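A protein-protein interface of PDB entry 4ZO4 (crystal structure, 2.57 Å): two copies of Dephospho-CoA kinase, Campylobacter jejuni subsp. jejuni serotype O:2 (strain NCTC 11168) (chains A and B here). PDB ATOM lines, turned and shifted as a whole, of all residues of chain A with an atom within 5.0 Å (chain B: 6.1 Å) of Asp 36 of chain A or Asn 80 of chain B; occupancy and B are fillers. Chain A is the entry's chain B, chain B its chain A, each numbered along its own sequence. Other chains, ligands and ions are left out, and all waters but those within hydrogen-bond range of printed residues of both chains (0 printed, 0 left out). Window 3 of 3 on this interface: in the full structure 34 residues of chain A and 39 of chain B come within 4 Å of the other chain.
N of Lys 82 of chain B sits at hydrogen-bond distance from O of Leu 120 of chain A, 2.8 Å away.
ND2 of Asn 80 of chain B lies within hydrogen-bond range of O of Glu 76 of chain B (2.9 Å).
Among the printed residues, merely in contact across the chains: Asp 36 of chain A with Asn 80 of chain B, Ala 39 of chain A with Phe 79 of chain B, Leu 120 of chain A with Asn 80 of chain B, Leu 120 of chain A with Asn 81 of chain B and Phe 121 of chain A with Asn 80 of chain B.
Printed residues of chain B within 4 Å of Asp 36 of chain A: Asn 80 (3.2 Å).
Asn 80 of chain B touches three residues of chain A.
Printed residues of chain A within 4 Å of Phe 79 of chain B: Ala 39.
Of the printed residues of chain A, Lys 82 of chain B touches Leu 120.
His 40 of chain A touches none of the printed residues of chain B.
Of the 9 printed residues of chain A, 4 touch a printed residue of chain B.
Printed residues of chain A that touch a printed residue of chain B: Asp 36, Ala 39, Leu 120 and Phe 121.
Hydrophobic or aromatic side chains of chain A that line the printed part of chain B: Ala 39, Leu 120 and Phe 121.
No position is printed for both chains.
Of the 6 pairs that touch across the chains among the printed residues, none has its exchanged pair printed and touching as well.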
ATOM      1  N   SER A  34      34.083 -17.988 -15.108  1.00  0.00           N
ATOM      2  CA  SER A  34      33.308 -17.896 -13.864  1.00  0.00           C
ATOM      3  C   SER A  34      32.193 -16.893 -14.086  1.00  0.00           C
ATOM      4  O   SER A  34      32.448 -15.758 -14.444  1.00  0.00           O
ATOM      5  CB  SER A  34      34.206 -17.475 -12.713  1.00  0.00           C
ATOM      6  OG  SER A  34      33.458 -17.262 -11.548  1.00  0.00           O
ATOM      7  N   ALA A  35      30.952 -17.336 -13.942  1.00  0.00           N
ATOM      8  CA  ALA A  35      29.807 -16.421 -14.015  1.00  0.00           C
ATOM      9  C   ALA A  35      29.926 -15.365 -12.906  1.00  0.00           C
ATOM     10  O   ALA A  35      29.786 -14.185 -13.161  1.00  0.00           O
ATOM     11  CB  ALA A  35      28.505 -17.189 -13.872  1.00  0.00           C
ATOM     12  N   ASP A  36      30.208 -15.822 -11.689  1.00  0.00           N
ATOM     13  CA  ASP A  36      30.283 -14.971 -10.516  1.00  0.00           C
ATOM     14  C   ASP A  36      31.319 -13.854 -10.696  1.00  0.00           C
ATOM     15  O   ASP A  36      31.065 -12.702 -10.333  1.00  0.00           O
ATOM     16  CB  ASP A  36      30.592 -15.823  -9.283  1.00  0.00           C
ATOM     17  CG  ASP A  36      29.455 -16.807  -8.935  1.00  0.00           C
ATOM     18  OD1 ASP A  36      28.322 -16.614  -9.425  1.00  0.00           O
ATOM     19  OD2 ASP A  36      29.690 -17.772  -8.160  1.00  0.00           O
ATOM     20  N   LYS A  37      32.462 -14.192 -11.290  1.00  0.00           N
ATOM     21  CA  LYS A  37      33.506 -13.214 -11.591  1.00  0.00           C
ATOM     22  C   LYS A  37      33.134 -12.223 -12.685  1.00  0.00           C
ATOM     23  O   LYS A  37      33.442 -11.030 -12.583  1.00  0.00           O
ATOM     24  CB  LYS A  37      34.799 -13.907 -12.020  1.00  0.00           C
ATOM     25  CG  LYS A  37      36.031 -13.056 -11.714  1.00  0.00           C
ATOM     26  CD  LYS A  37      37.005 -12.966 -12.885  1.00  0.00           C
ATOM     27  CE  LYS A  37      38.199 -12.105 -12.497  1.00  0.00           C
ATOM     28  NZ  LYS A  37      39.089 -11.797 -13.657  1.00  0.00           N
ATOM     29  N   ILE A  38      32.524 -12.715 -13.759  1.00  0.00           N
ATOM     30  CA  ILE A  38      32.038 -11.832 -14.807  1.00  0.00           C
ATOM     31  C   ILE A  38      31.078 -10.813 -14.185  1.00  0.00           C
ATOM     32  O   ILE A  38      31.200  -9.617 -14.431  1.00  0.00           O
ATOM     33  CB  ILE A  38      31.282 -12.586 -15.914  1.00  0.00           C
ATOM     34  CG1 ILE A  38      32.172 -13.612 -16.643  1.00  0.00           C
ATOM     35  CG2 ILE A  38      30.723 -11.610 -16.939  1.00  0.00           C
ATOM     36  CD1 ILE A  38      33.212 -13.012 -17.564  1.00  0.00           C
ATOM     37  N   ALA A  39      30.145 -11.273 -13.355  1.00  0.00           N
ATOM     38  CA  ALA A  39      29.172 -10.368 -12.789  1.00  0.00           C
ATOM     39  C   ALA A  39      29.894  -9.309 -11.951  1.00  0.00           C
ATOM     40  O   ALA A  39      29.674  -8.111 -12.106  1.00  0.00           O
ATOM     41  CB  ALA A  39      28.153 -11.125 -11.956  1.00  0.00           C
ATOM     42  N   HIS A  40      30.764  -9.766 -11.068  1.00  0.00           N
ATOM     43  CA  HIS A  40      31.588  -8.879 -10.268  1.00  0.00           C
ATOM     44  C   HIS A  40      32.185  -7.755 -11.125  1.00  0.00           C
ATOM     45  O   HIS A  40      32.107  -6.593 -10.763  1.00  0.00           O
ATOM     46  CB  HIS A  40      32.694  -9.710  -9.619  1.00  0.00           C
ATOM     47  CG  HIS A  40      33.413  -9.014  -8.512  1.00  0.00           C
ATOM     48  ND1 HIS A  40      33.774  -7.683  -8.570  1.00  0.00           N
ATOM     49  CD2 HIS A  40      33.878  -9.481  -7.330  1.00  0.00           C
ATOM     50  CE1 HIS A  40      34.408  -7.356  -7.459  1.00  0.00           C
ATOM     51  NE2 HIS A  40      34.486  -8.428  -6.691  1.00  0.00           N
ATOM     52  N   LEU A 120      24.188 -19.586 -11.859  1.00  0.00           N
ATOM     53  CA  LEU A 120      23.038 -19.996 -11.046  1.00  0.00           C
ATOM     54  C   LEU A 120      22.019 -18.854 -10.668  1.00  0.00           C
ATOM     55  O   LEU A 120      21.222 -19.034  -9.763  1.00  0.00           O
ATOM     56  CB  LEU A 120      23.544 -20.733  -9.803  1.00  0.00           C
ATOM     57  CG  LEU A 120      24.081 -22.151 -10.033  1.00  0.00           C
ATOM     58  CD1 LEU A 120      24.663 -22.732  -8.749  1.00  0.00           C
ATOM     59  CD2 LEU A 120      22.961 -23.038 -10.577  1.00  0.00           C
ATOM     60  N   PHE A 121      22.027 -17.722 -11.387  1.00  0.00           N
ATOM     61  CA  PHE A 121      20.915 -16.748 -11.370  1.00  0.00           C
ATOM     62  C   PHE A 121      20.109 -16.932 -12.662  1.00  0.00           C
ATOM     63  O   PHE A 121      19.748 -15.979 -13.362  1.00  0.00           O
ATOM     64  CB  PHE A 121      21.414 -15.292 -11.214  1.00  0.00           C
ATOM     65  CG  PHE A 121      22.503 -14.920 -12.174  1.00  0.00           C
ATOM     66  CD1 PHE A 121      22.201 -14.426 -13.440  1.00  0.00           C
ATOM     67  CD2 PHE A 121      23.833 -15.102 -11.827  1.00  0.00           C
ATOM     68  CE1 PHE A 121      23.204 -14.121 -14.338  1.00  0.00           C
ATOM     69  CE2 PHE A 121      24.843 -14.799 -12.714  1.00  0.00           C
ATOM     70  CZ  PHE A 121      24.526 -14.307 -13.967  1.00  0.00           C
ATOM     71  N   GLY B  75      25.050 -10.972   0.541  1.00  0.00           N
ATOM     72  CA  GLY B  75      24.570 -10.317  -0.675  1.00  0.00           C
ATOM     73  C   GLY B  75      25.231 -10.789  -1.979  1.00  0.00           C
ATOM     74  O   GLY B  75      24.590 -10.815  -3.033  1.00  0.00           O
ATOM     75  N   GLU B  76      26.503 -11.175  -1.932  1.00  0.00           N
ATOM     76  CA  GLU B  76      27.134 -11.744  -3.119  1.00  0.00           C
ATOM     77  C   GLU B  76      26.513 -13.087  -3.425  1.00  0.00           C
ATOM     78  O   GLU B  76      26.320 -13.433  -4.592  1.00  0.00           O
ATOM     79  CB  GLU B  76      28.645 -11.883  -2.947  1.00  0.00           C
ATOM     80  CG  GLU B  76      29.337 -10.516  -2.884  1.00  0.00           C
ATOM     81  CD  GLU B  76      30.841 -10.576  -2.622  1.00  0.00           C
ATOM     82  OE1 GLU B  76      31.444  -9.484  -2.506  1.00  0.00           O
ATOM     83  OE2 GLU B  76      31.412 -11.688  -2.524  1.00  0.00           O
ATOM     84  N   ILE B  77      26.196 -13.845  -2.380  1.00  0.00           N
ATOM     85  CA  ILE B  77      25.635 -15.169  -2.587  1.00  0.00           C
ATOM     86  C   ILE B  77      24.284 -15.048  -3.292  1.00  0.00           C
ATOM     87  O   ILE B  77      24.057 -15.683  -4.319  1.00  0.00           O
ATOM     88  CB  ILE B  77      25.457 -15.927  -1.258  1.00  0.00           C
ATOM     89  CG1 ILE B  77      26.791 -16.415  -0.727  1.00  0.00           C
ATOM     90  CG2 ILE B  77      24.527 -17.108  -1.429  1.00  0.00           C
ATOM     91  CD1 ILE B  77      26.667 -17.140   0.591  1.00  0.00           C
ATOM     92  N   VAL B  78      23.412 -14.206  -2.739  1.00  0.00           N
ATOM     93  CA  VAL B  78      22.041 -14.079  -3.242  1.00  0.00           C
ATOM     94  C   VAL B  78      22.018 -13.308  -4.566  1.00  0.00           C
ATOM     95  O   VAL B  78      21.094 -13.443  -5.357  1.00  0.00           O
ATOM     96  CB  VAL B  78      21.046 -13.415  -2.211  1.00  0.00           C
ATOM     97  CG1 VAL B  78      20.784 -14.340  -1.047  1.00  0.00           C
ATOM     98  CG2 VAL B  78      21.555 -12.074  -1.720  1.00  0.00           C
ATOM     99  N   PHE B  79      23.010 -12.479  -4.807  1.00  0.00           N
ATOM    100  CA  PHE B  79      23.091 -11.876  -6.128  1.00  0.00           C
ATOM    101  C   PHE B  79      23.512 -12.947  -7.158  1.00  0.00           C
ATOM    102  O   PHE B  79      22.946 -13.014  -8.240  1.00  0.00           O
ATOM    103  CB  PHE B  79      24.048 -10.678  -6.142  1.00  0.00           C
ATOM    104  CG  PHE B  79      24.240 -10.088  -7.510  1.00  0.00           C
ATOM    105  CD1 PHE B  79      23.230  -9.324  -8.110  1.00  0.00           C
ATOM    106  CD2 PHE B  79      25.422 -10.327  -8.222  1.00  0.00           C
ATOM    107  CE1 PHE B  79      23.401  -8.807  -9.391  1.00  0.00           C
ATOM    108  CE2 PHE B  79      25.593  -9.808  -9.500  1.00  0.00           C
ATOM    109  CZ  PHE B  79      24.582  -9.050 -10.086  1.00  0.00           C
ATOM    110  N   ASN B  80      24.468 -13.801  -6.804  1.00  0.00           N
ATOM    111  CA  ASN B  80      24.935 -14.879  -7.710  1.00  0.00           C
ATOM    112  C   ASN B  80      24.066 -16.120  -7.798  1.00  0.00           C
ATOM    113  O   ASN B  80      24.295 -16.968  -8.656  1.00  0.00           O
ATOM    114  CB  ASN B  80      26.314 -15.368  -7.284  1.00  0.00           C
ATOM    115  CG  ASN B  80      27.341 -14.274  -7.317  1.00  0.00           C
ATOM    116  OD1 ASN B  80      27.238 -13.329  -8.103  1.00  0.00           O
ATOM    117  ND2 ASN B  80      28.322 -14.374  -6.437  1.00  0.00           N
ATOM    118  N   ASN B  81      23.093 -16.252  -6.907  1.00  0.00           N
ATOM    119  CA  ASN B  81      22.346 -17.492  -6.823  1.00  0.00           C
ATOM    120  C   ASN B  81      20.886 -17.236  -6.576  1.00  0.00           C
ATOM    121  O   ASN B  81      20.502 -16.632  -5.559  1.00  0.00           O
ATOM    122  CB  ASN B  81      22.933 -18.344  -5.714  1.00  0.00           C
ATOM    123  CG  ASN B  81      22.507 -19.766  -5.806  1.00  0.00           C
ATOM    124  OD1 ASN B  81      21.351 -20.101  -5.533  1.00  0.00           O
ATOM    125  ND2 ASN B  81      23.439 -20.628  -6.186  1.00  0.00           N
ATOM    126  N   LYS B  82      20.079 -17.695  -7.522  1.00  0.00           N
ATOM    127  CA  LYS B  82      18.621 -17.588  -7.487  1.00  0.00           C
ATOM    128  C   LYS B  82      18.006 -18.371  -6.313  1.00  0.00           C
ATOM    129  O   LYS B  82      17.057 -17.936  -5.671  1.00  0.00           O
ATOM    130  CB  LYS B  82      18.061 -18.092  -8.822  1.00  0.00           C
ATOM    131  CG  LYS B  82      16.680 -17.591  -9.227  1.00  0.00           C
ATOM    132  CD  LYS B  82      16.388 -17.959 -10.684  1.00  0.00           C
ATOM    133  CE  LYS B  82      14.985 -17.554 -11.131  1.00  0.00           C
ATOM    134  NZ  LYS B  82      14.762 -17.805 -12.587  1.00  0.00           N
